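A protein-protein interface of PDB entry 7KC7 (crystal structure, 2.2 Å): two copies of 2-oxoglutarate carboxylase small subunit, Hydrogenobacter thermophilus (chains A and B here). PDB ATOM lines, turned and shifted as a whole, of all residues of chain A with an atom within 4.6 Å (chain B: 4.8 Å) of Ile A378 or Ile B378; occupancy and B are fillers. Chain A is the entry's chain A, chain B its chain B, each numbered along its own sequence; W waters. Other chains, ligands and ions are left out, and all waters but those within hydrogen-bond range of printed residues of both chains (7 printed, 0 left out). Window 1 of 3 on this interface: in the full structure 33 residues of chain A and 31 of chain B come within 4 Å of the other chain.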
ATOM      1  N   ARG A  32     -24.178   3.199  17.712  1.00  0.00           N
ATOM      2  CA  ARG A  32     -23.063   3.744  18.470  1.00  0.00           C
ATOM      3  C   ARG A  32     -22.165   4.590  17.555  1.00  0.00           C
ATOM      4  O   ARG A  32     -21.802   5.713  17.901  1.00  0.00           O
ATOM      5  CB  ARG A  32     -22.282   2.619  19.185  1.00  0.00           C
ATOM      6  CG  ARG A  32     -21.064   3.088  19.999  1.00  0.00           C
ATOM      7  CD  ARG A  32     -20.444   2.005  20.905  1.00  0.00           C
ATOM      8  NE  ARG A  32     -21.476   1.363  21.725  1.00  0.00           N
ATOM      9  CZ  ARG A  32     -22.142   2.032  22.658  1.00  0.00           C
ATOM     10  NH1 ARG A  32     -21.888   3.327  22.854  1.00  0.00           N
ATOM     11  NH2 ARG A  32     -23.075   1.448  23.355  1.00  0.00           N
ATOM     12  N   PRO A 373     -17.982 -10.668  30.214  1.00  0.00           N
ATOM     13  CA  PRO A 373     -16.619 -10.411  30.644  1.00  0.00           C
ATOM     14  C   PRO A 373     -16.071  -9.131  30.014  1.00  0.00           C
ATOM     15  O   PRO A 373     -16.539  -8.675  28.961  1.00  0.00           O
ATOM     16  CB  PRO A 373     -15.882 -11.670  30.174  1.00  0.00           C
ATOM     17  CG  PRO A 373     -16.639 -12.147  29.043  1.00  0.00           C
ATOM     18  CD  PRO A 373     -18.069 -11.735  29.202  1.00  0.00           C
ATOM     19  N   GLY A 374     -15.103  -8.536  30.722  1.00  0.00           N
ATOM     20  CA  GLY A 374     -14.426  -7.321  30.311  1.00  0.00           C
ATOM     21  C   GLY A 374     -13.014  -7.311  30.865  1.00  0.00           C
ATOM     22  O   GLY A 374     -12.711  -8.039  31.820  1.00  0.00           O
ATOM     23  N   GLY A 375     -12.159  -6.479  30.275  1.00  0.00           N
ATOM     24  CA  GLY A 375     -10.779  -6.377  30.710  1.00  0.00           C
ATOM     25  C   GLY A 375      -9.866  -5.839  29.611  1.00  0.00           C
ATOM     26  O   GLY A 375     -10.310  -5.416  28.540  1.00  0.00           O
ATOM     27  N   PHE A 376      -8.568  -5.866  29.917  1.00  0.00           N
ATOM     28  CA  PHE A 376      -7.545  -5.450  28.967  1.00  0.00           C
ATOM     29  C   PHE A 376      -7.648  -6.298  27.705  1.00  0.00           C
ATOM     30  O   PHE A 376      -7.645  -7.528  27.777  1.00  0.00           O
ATOM     31  CB  PHE A 376      -6.170  -5.607  29.622  1.00  0.00           C
ATOM     32  CG  PHE A 376      -5.000  -5.224  28.738  1.00  0.00           C
ATOM     33  CD1 PHE A 376      -4.487  -6.128  27.813  1.00  0.00           C
ATOM     34  CD2 PHE A 376      -4.384  -3.999  28.868  1.00  0.00           C
ATOM     35  CE1 PHE A 376      -3.392  -5.791  27.000  1.00  0.00           C
ATOM     36  CE2 PHE A 376      -3.292  -3.656  28.076  1.00  0.00           C
ATOM     37  CZ  PHE A 376      -2.791  -4.548  27.152  1.00  0.00           C
ATOM     38  N   GLY A 377      -7.778  -5.637  26.555  1.00  0.00           N
ATOM     39  CA  GLY A 377      -7.843  -6.349  25.295  1.00  0.00           C
ATOM     40  C   GLY A 377      -9.129  -7.108  25.050  1.00  0.00           C
ATOM     41  O   GLY A 377      -9.133  -8.044  24.248  1.00  0.00           O
ATOM     42  N   ILE A 378     -10.227  -6.749  25.701  1.00  0.00           N
ATOM     43  CA  ILE A 378     -11.490  -7.431  25.471  1.00  0.00           C
ATOM     44  C   ILE A 378     -12.546  -6.447  24.985  1.00  0.00           C
ATOM     45  O   ILE A 378     -12.810  -5.416  25.628  1.00  0.00           O
ATOM     46  CB  ILE A 378     -11.990  -8.178  26.721  1.00  0.00           C
ATOM     47  CG1 ILE A 378     -11.020  -9.310  27.090  1.00  0.00           C
ATOM     48  CG2 ILE A 378     -13.407  -8.689  26.449  1.00  0.00           C
ATOM     49  CD1 ILE A 378     -11.284  -9.870  28.521  1.00  0.00           C
ATOM     50  N   ARG A 379     -13.225  -6.831  23.923  1.00  0.00           N
ATOM     51  CA  ARG A 379     -14.320  -6.079  23.338  1.00  0.00           C
ATOM     52  C   ARG A 379     -15.491  -7.036  23.215  1.00  0.00           C
ATOM     53  O   ARG A 379     -15.307  -8.202  22.850  1.00  0.00           O
ATOM     54  CB  ARG A 379     -13.937  -5.541  21.949  1.00  0.00           C
ATOM     55  CG  ARG A 379     -15.055  -4.867  21.194  1.00  0.00           C
ATOM     56  CD  ARG A 379     -14.494  -4.318  19.885  1.00  0.00           C
ATOM     57  NE  ARG A 379     -15.548  -3.801  19.008  1.00  0.00           N
ATOM     58  CZ  ARG A 379     -15.337  -3.323  17.786  1.00  0.00           C
ATOM     59  NH1 ARG A 379     -14.110  -3.301  17.280  1.00  0.00           N
ATOM     60  NH2 ARG A 379     -16.339  -2.838  17.072  1.00  0.00           N
ATOM     61  N   VAL A 380     -16.690  -6.546  23.485  1.00  0.00           N
ATOM     62  CA  VAL A 380     -17.904  -7.341  23.376  1.00  0.00           C
ATOM     63  C   VAL A 380     -18.906  -6.572  22.542  1.00  0.00           C
ATOM     64  O   VAL A 380     -19.133  -5.386  22.790  1.00  0.00           O
ATOM     65  CB  VAL A 380     -18.513  -7.682  24.746  1.00  0.00           C
ATOM     66  CG1 VAL A 380     -19.819  -8.532  24.587  1.00  0.00           C
ATOM     67  CG2 VAL A 380     -17.493  -8.406  25.599  1.00  0.00           C
ATOM     68  N   LEU A 401     -17.696 -11.968  21.081  1.00  0.00           N
ATOM     69  CA  LEU A 401     -16.596 -11.754  21.998  1.00  0.00           C
ATOM     70  C   LEU A 401     -15.336 -11.586  21.172  1.00  0.00           C
ATOM     71  O   LEU A 401     -15.017 -12.453  20.347  1.00  0.00           O
ATOM     72  CB  LEU A 401     -16.481 -12.937  22.953  1.00  0.00           C
ATOM     73  CG  LEU A 401     -15.381 -12.915  24.011  1.00  0.00           C
ATOM     74  CD1 LEU A 401     -15.406 -11.622  24.804  1.00  0.00           C
ATOM     75  CD2 LEU A 401     -15.613 -14.183  24.896  1.00  0.00           C
ATOM     76  N   ILE A 402     -14.662 -10.456  21.333  1.00  0.00           N
ATOM     77  CA  ILE A 402     -13.481 -10.116  20.542  1.00  0.00           C
ATOM     78  C   ILE A 402     -12.328  -9.781  21.467  1.00  0.00           C
ATOM     79  O   ILE A 402     -12.513  -9.068  22.463  1.00  0.00           O
ATOM     80  CB  ILE A 402     -13.772  -8.928  19.609  1.00  0.00           C
ATOM     81  CG1 ILE A 402     -14.958  -9.250  18.674  1.00  0.00           C
ATOM     82  CG2 ILE A 402     -12.522  -8.546  18.833  1.00  0.00           C
ATOM     83  CD1 ILE A 402     -16.058  -8.167  18.796  1.00  0.00           C
ATOM     84  N   VAL A 403     -11.136 -10.302  21.156  1.00  0.00           N
ATOM     85  CA  VAL A 403      -9.951 -10.067  21.979  1.00  0.00           C
ATOM     86  C   VAL A 403      -8.816  -9.621  21.083  1.00  0.00           C
ATOM     87  O   VAL A 403      -8.802  -9.881  19.884  1.00  0.00           O
ATOM     88  CB  VAL A 403      -9.498 -11.285  22.815  1.00  0.00           C
ATOM     89  CG1 VAL A 403     -10.630 -11.775  23.721  1.00  0.00           C
ATOM     90  CG2 VAL A 403      -8.947 -12.363  21.868  1.00  0.00           C
ATOM     91  N   ARG A 414      -6.218 -15.156  26.186  1.00  0.00           N
ATOM     92  CA  ARG A 414      -7.176 -14.117  26.548  1.00  0.00           C
ATOM     93  C   ARG A 414      -8.618 -14.486  26.168  1.00  0.00           C
ATOM     94  O   ARG A 414      -9.564 -14.174  26.915  1.00  0.00           O
ATOM     95  CB  ARG A 414      -6.764 -12.816  25.899  1.00  0.00           C
ATOM     96  CG  ARG A 414      -7.728 -11.749  26.169  1.00  0.00           C
ATOM     97  CD  ARG A 414      -7.018 -10.439  25.933  1.00  0.00           C
ATOM     98  NE  ARG A 414      -6.041 -10.212  27.007  1.00  0.00           N
ATOM     99  CZ  ARG A 414      -4.939  -9.462  26.913  1.00  0.00           C
ATOM    100  NH1 ARG A 414      -4.619  -8.843  25.766  1.00  0.00           N
ATOM    101  NH2 ARG A 414      -4.151  -9.330  27.989  1.00  0.00           N
ATOM    102  N   ALA A 418     -11.559 -15.343  28.649  1.00  0.00           N
ATOM    103  CA  ALA A 418     -12.788 -14.552  28.604  1.00  0.00           C
ATOM    104  C   ALA A 418     -14.000 -15.462  28.491  1.00  0.00           C
ATOM    105  O   ALA A 418     -15.032 -15.239  29.146  1.00  0.00           O
ATOM    106  CB  ALA A 418     -12.702 -13.531  27.459  1.00  0.00           C
ATOM    107  N   ARG B  32      -8.486 -12.495  36.128  1.00  0.00           N
ATOM    108  CA  ARG B  32      -8.356 -12.587  34.670  1.00  0.00           C
ATOM    109  C   ARG B  32      -6.884 -12.598  34.273  1.00  0.00           C
ATOM    110  O   ARG B  32      -6.445 -13.461  33.519  1.00  0.00           O
ATOM    111  CB  ARG B  32      -9.104 -11.427  33.992  1.00  0.00           C
ATOM    112  CG  ARG B  32      -9.031 -11.429  32.452  1.00  0.00           C
ATOM    113  CD  ARG B  32     -10.083 -10.534  31.755  1.00  0.00           C
ATOM    114  NE  ARG B  32     -11.425 -10.768  32.263  1.00  0.00           N
ATOM    115  CZ  ARG B  32     -12.096 -11.908  32.100  1.00  0.00           C
ATOM    116  NH1 ARG B  32     -11.531 -12.939  31.433  1.00  0.00           N
ATOM    117  NH2 ARG B  32     -13.318 -12.023  32.627  1.00  0.00           N
ATOM    118  N   PRO B 373     -22.498  -1.609  27.992  1.00  0.00           N
ATOM    119  CA  PRO B 373     -22.172  -1.246  26.609  1.00  0.00           C
ATOM    120  C   PRO B 373     -20.863  -1.853  26.134  1.00  0.00           C
ATOM    121  O   PRO B 373     -20.021  -2.273  26.923  1.00  0.00           O
ATOM    122  CB  PRO B 373     -22.074   0.281  26.655  1.00  0.00           C
ATOM    123  CG  PRO B 373     -21.739   0.608  28.077  1.00  0.00           C
ATOM    124  CD  PRO B 373     -22.314  -0.482  28.937  1.00  0.00           C
ATOM    125  N   GLY B 374     -20.736  -1.979  24.821  1.00  0.00           N
ATOM    126  CA  GLY B 374     -19.528  -2.532  24.243  1.00  0.00           C
ATOM    127  C   GLY B 374     -19.319  -1.919  22.886  1.00  0.00           C
ATOM    128  O   GLY B 374     -20.249  -1.377  22.288  1.00  0.00           O
ATOM    129  N   GLY B 375     -18.093  -2.024  22.402  1.00  0.00           N
ATOM    130  CA  GLY B 375     -17.753  -1.496  21.099  1.00  0.00           C
ATOM    131  C   GLY B 375     -16.282  -1.163  20.993  1.00  0.00           C
ATOM    132  O   GLY B 375     -15.478  -1.387  21.917  1.00  0.00           O
ATOM    133  N   PHE B 376     -15.971  -0.591  19.837  1.00  0.00           N
ATOM    134  CA  PHE B 376     -14.658  -0.123  19.467  1.00  0.00           C
ATOM    135  C   PHE B 376     -14.204   0.934  20.459  1.00  0.00           C
ATOM    136  O   PHE B 376     -14.909   1.913  20.718  1.00  0.00           O
ATOM    137  CB  PHE B 376     -14.760   0.460  18.046  1.00  0.00           C
ATOM    138  CG  PHE B 376     -13.462   0.949  17.470  1.00  0.00           C
ATOM    139  CD1 PHE B 376     -12.988   2.228  17.766  1.00  0.00           C
ATOM    140  CD2 PHE B 376     -12.717   0.147  16.635  1.00  0.00           C
ATOM    141  CE1 PHE B 376     -11.781   2.668  17.247  1.00  0.00           C
ATOM    142  CE2 PHE B 376     -11.513   0.601  16.080  1.00  0.00           C
ATOM    143  CZ  PHE B 376     -11.056   1.859  16.398  1.00  0.00           C
ATOM    144  N   GLY B 377     -13.048   0.708  21.043  1.00  0.00           N
ATOM    145  CA  GLY B 377     -12.515   1.617  22.030  1.00  0.00           C
ATOM    146  C   GLY B 377     -13.220   1.626  23.353  1.00  0.00           C
ATOM    147  O   GLY B 377     -12.988   2.550  24.150  1.00  0.00           O
ATOM    148  N   ILE B 378     -13.979   0.575  23.679  1.00  0.00           N
ATOM    149  CA  ILE B 378     -14.717   0.521  24.939  1.00  0.00           C
ATOM    150  C   ILE B 378     -14.295  -0.684  25.769  1.00  0.00           C
ATOM    151  O   ILE B 378     -14.364  -1.826  25.296  1.00  0.00           O
ATOM    152  CB  ILE B 378     -16.235   0.479  24.702  1.00  0.00           C
ATOM    153  CG1 ILE B 378     -16.682   1.740  23.958  1.00  0.00           C
ATOM    154  CG2 ILE B 378     -16.953   0.332  26.076  1.00  0.00           C
ATOM    155  CD1 ILE B 378     -18.126   1.738  23.478  1.00  0.00           C
ATOM    156  N   ARG B 379     -13.976  -0.441  27.039  1.00  0.00           N
ATOM    157  CA  ARG B 379     -13.571  -1.472  27.987  1.00  0.00           C
ATOM    158  C   ARG B 379     -14.404  -1.340  29.245  1.00  0.00           C
ATOM    159  O   ARG B 379     -14.636  -0.220  29.727  1.00  0.00           O
ATOM    160  CB  ARG B 379     -12.078  -1.322  28.322  1.00  0.00           C
ATOM    161  CG  ARG B 379     -11.561  -2.206  29.410  1.00  0.00           C
ATOM    162  CD  ARG B 379     -10.052  -2.010  29.546  1.00  0.00           C
ATOM    163  NE  ARG B 379      -9.597  -2.654  30.789  1.00  0.00           N
ATOM    164  CZ  ARG B 379      -8.334  -2.681  31.195  1.00  0.00           C
ATOM    165  NH1 ARG B 379      -7.396  -2.098  30.463  1.00  0.00           N
ATOM    166  NH2 ARG B 379      -7.997  -3.291  32.343  1.00  0.00           N
ATOM    167  N   VAL B 380     -14.791  -2.485  29.823  1.00  0.00           N
ATOM    168  CA  VAL B 380     -15.608  -2.485  31.023  1.00  0.00           C
ATOM    169  C   VAL B 380     -14.972  -3.399  32.041  1.00  0.00           C
ATOM    170  O   VAL B 380     -14.690  -4.572  31.758  1.00  0.00           O
ATOM    171  CB  VAL B 380     -17.062  -2.902  30.759  1.00  0.00           C
ATOM    172  CG1 VAL B 380     -17.852  -2.815  32.073  1.00  0.00           C
ATOM    173  CG2 VAL B 380     -17.661  -1.996  29.655  1.00  0.00           C
ATOM    174  N   LEU B 401     -16.248   2.225  33.541  1.00  0.00           N
ATOM    175  CA  LEU B 401     -16.442   2.332  32.097  1.00  0.00           C
ATOM    176  C   LEU B 401     -15.223   3.054  31.532  1.00  0.00           C
ATOM    177  O   LEU B 401     -14.943   4.179  31.942  1.00  0.00           O
ATOM    178  CB  LEU B 401     -17.741   3.087  31.797  1.00  0.00           C
ATOM    179  CG  LEU B 401     -18.013   3.337  30.305  1.00  0.00           C
ATOM    180  CD1 LEU B 401     -18.087   1.912  29.625  1.00  0.00           C
ATOM    181  CD2 LEU B 401     -19.301   4.159  30.101  1.00  0.00           C
ATOM    182  N   ILE B 402     -14.495   2.408  30.613  1.00  0.00           N
ATOM    183  CA  ILE B 402     -13.237   2.939  30.103  1.00  0.00           C
ATOM    184  C   ILE B 402     -13.307   3.054  28.581  1.00  0.00           C
ATOM    185  O   ILE B 402     -13.814   2.154  27.884  1.00  0.00           O
ATOM    186  CB  ILE B 402     -12.031   2.078  30.538  1.00  0.00           C
ATOM    187  CG1 ILE B 402     -11.999   1.914  32.061  1.00  0.00           C
ATOM    188  CG2 ILE B 402     -10.684   2.686  30.070  1.00  0.00           C
ATOM    189  CD1 ILE B 402     -11.958   0.478  32.512  1.00  0.00           C
ATOM    190  N   VAL B 403     -12.787   4.172  28.069  1.00  0.00           N
ATOM    191  CA  VAL B 403     -12.830   4.483  26.646  1.00  0.00           C
ATOM    192  C   VAL B 403     -11.453   4.920  26.134  1.00  0.00           C
ATOM    193  O   VAL B 403     -10.640   5.503  26.856  1.00  0.00           O
ATOM    194  CB  VAL B 403     -13.896   5.571  26.458  1.00  0.00           C
ATOM    195  CG1 VAL B 403     -13.611   6.358  25.302  1.00  0.00           C
ATOM    196  CG2 VAL B 403     -15.254   4.934  26.454  1.00  0.00           C
ATOM    197  N   ARG B 414     -17.225   9.276  22.683  1.00  0.00           N
ATOM    198  CA  ARG B 414     -17.344   7.844  22.942  1.00  0.00           C
ATOM    199  C   ARG B 414     -17.811   7.577  24.367  1.00  0.00           C
ATOM    200  O   ARG B 414     -18.776   6.823  24.579  1.00  0.00           O
ATOM    201  CB  ARG B 414     -15.981   7.204  22.659  1.00  0.00           C
ATOM    202  CG  ARG B 414     -15.899   5.746  22.886  1.00  0.00           C
ATOM    203  CD  ARG B 414     -14.730   5.173  22.079  1.00  0.00           C
ATOM    204  NE  ARG B 414     -15.018   5.220  20.658  1.00  0.00           N
ATOM    205  CZ  ARG B 414     -14.123   5.216  19.669  1.00  0.00           C
ATOM    206  NH1 ARG B 414     -12.819   5.164  19.909  1.00  0.00           N
ATOM    207  NH2 ARG B 414     -14.571   5.258  18.409  1.00  0.00           N
ATOM    208  N   ALA B 418     -21.235   5.888  25.333  1.00  0.00           N
ATOM    209  CA  ALA B 418     -21.299   4.635  26.097  1.00  0.00           C
ATOM    210  C   ALA B 418     -22.180   4.781  27.335  1.00  0.00           C
ATOM    211  O   ALA B 418     -23.052   3.940  27.606  1.00  0.00           O
ATOM    212  CB  ALA B 418     -19.891   4.188  26.506  1.00  0.00           C
HETATM  213  O   HOH W   1     -13.806  -4.948  28.249  1.00  0.00           O
HETATM  214  O   HOH W   2     -14.688  -9.736  33.602  1.00  0.00           O
HETATM  215  O   HOH W   3      -9.207 -12.944  29.301  1.00  0.00           O
HETATM  216  O   HOH W   4     -19.712   4.854  22.499  1.00  0.00           O
HETATM  217  O   HOH W   5     -16.477  -3.400  24.353  1.00  0.00           O
HETATM  218  O   HOH W   6     -11.581  -2.972  24.363  1.00  0.00           O
HETATM  219  O   HOH W   7     -15.063  -6.826  33.660  1.00  0.00           O
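Of the 14 printed residues of chain B, 9 touch a printed residue of chain A. Printed residues of chain B that touch a printed residue of chain A: Arg B32, Pro B373, Gly B374, Gly B375, Phe B376, Ile B378, Arg B379, Val B380 and Ala B418. Hydrophobic or aromatic side chains of chain B that line the printed part of chain A: Pro B373, Phe B376 and Ile B378. Of the 14 printed residues of chain A, 9 touch a printed residue of chain B.
Among the printed residues, merely in contact across the chains: Gly A374 with Val B380 (3.1 Å), Val A380 with Gly B374 (3.2 Å), Arg A379 with Gly B375 (3.4 Å), Gly A375 with Arg B379 (3.4 Å), Arg A32 with Ile B378 (3.5 Å), Ala A418 with Arg B32 (3.5 Å), Ile A378 with Arg B32 (3.5 Å), Val A380 with Gly B375 (3.5 Å), Arg A32 with Ala B418 (3.5 Å), Pro A373 with Arg B32 (3.6 Å), Arg A32 with Pro B373 (3.6 Å) and Ile A378 with Ile B378 (3.9 Å).
O of Ile A402 lies within hydrogen-bond range of N of Arg A379 (2.8 Å). N of Arg B379 sits at hydrogen-bond distance from O of Ile B402. The backbone carbonyl oxygen (O) of Phe B376 lies within hydrogen-bond range of the guanidinium group (NE) of Arg B414, 3.3 Å away. The guanidinium group (NE) of Arg A414 is in hydrogen-bond range of the backbone carbonyl oxygen (O) of Phe A376.
NE of Arg B379 lies close to N of Phe A376, 3.5 Å away. The guanidinium group (NE) of Arg A32 lies within hydrogen-bond range of the backbone carbonyl oxygen (O) of Gly B374 (3.1 Å). NE of Arg A379 sits close to N of Phe B376, 3.3 Å away. O of Val B380 is in hydrogen-bond range of N of Gly A375 (3.5 Å). The backbone carbonyl oxygen of Gly A374 sits at hydrogen-bond distance from the guanidinium group of Arg B32, 3.0 Å away.
Water W4 lies within hydrogen-bond range of NH1 of Arg A32 (2.7 Å), O of Arg B414 (3.0 Å) and N of Ala B418 (3.4 Å). Water W3 lies within hydrogen-bond range of the backbone carbonyl oxygen of Arg A414 (2.7 Å), the guanidinium group of Arg B32 (3.2 Å) and the backbone NH of Ala A418 (3.4 Å). Water W5 lies within hydrogen-bond range of the backbone carbonyl oxygen (O) of Ile B378, the backbone NH (N) of Gly B375 and the backbone NH (N) of Val A380. Water W2 lies within hydrogen-bond range of the guanidinium group (NH2) of Arg B32 (2.8 Å) and the backbone NH (N) of Gly A374 (3.1 Å). Water W1 lies within hydrogen-bond range of the backbone carbonyl oxygen of Ile A378 (2.8 Å), the backbone NH of Gly A375 (3.0 Å) and the backbone NH of Val B380 (3.1 Å). Water W6 bridges the backbone carbonyl oxygen of Ile A378 (3.0 Å) and the backbone carbonyl oxygen of Ile B378 (3.2 Å).
Arg A32 touches Ala B418, and with the chains exchanged Ala A418 touches Arg B32. Gly A375 touches Arg B379, and with the chains exchanged Arg A379 touches Gly B375. Gly A375 touches Val B380, and with the chains exchanged Val A380 touches Gly B375. Phe A376 touches Arg B379, and with the chains exchanged Arg A379 touches Phe B376. Of the 17 pairs that touch across the chains among the printed residues, 17 have their exchanged pair printed and touching as well.
Ile A378 touches just these residues of chain B: Arg B32 (3.5 Å) and Ile B378 (3.9 Å). Ile B378 touches two residues of chain A. Of the printed residues of chain B, Val A380 touches Gly B374 (3.2 Å) and Gly B375 (3.5 Å). Printed residues of chain A within 4 Å of Arg B379: Gly A375 (3.4 Å) and Phe A376 (3.4 Å). Gly B377 touches none of the printed residues of chain A. The nearest printed residue of chain A that does not touch Ile B378 is Arg A379 (4.7 Å). The nearest printed residue of chain B that does not touch Arg A379 is Ile B378 (4.7 Å).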
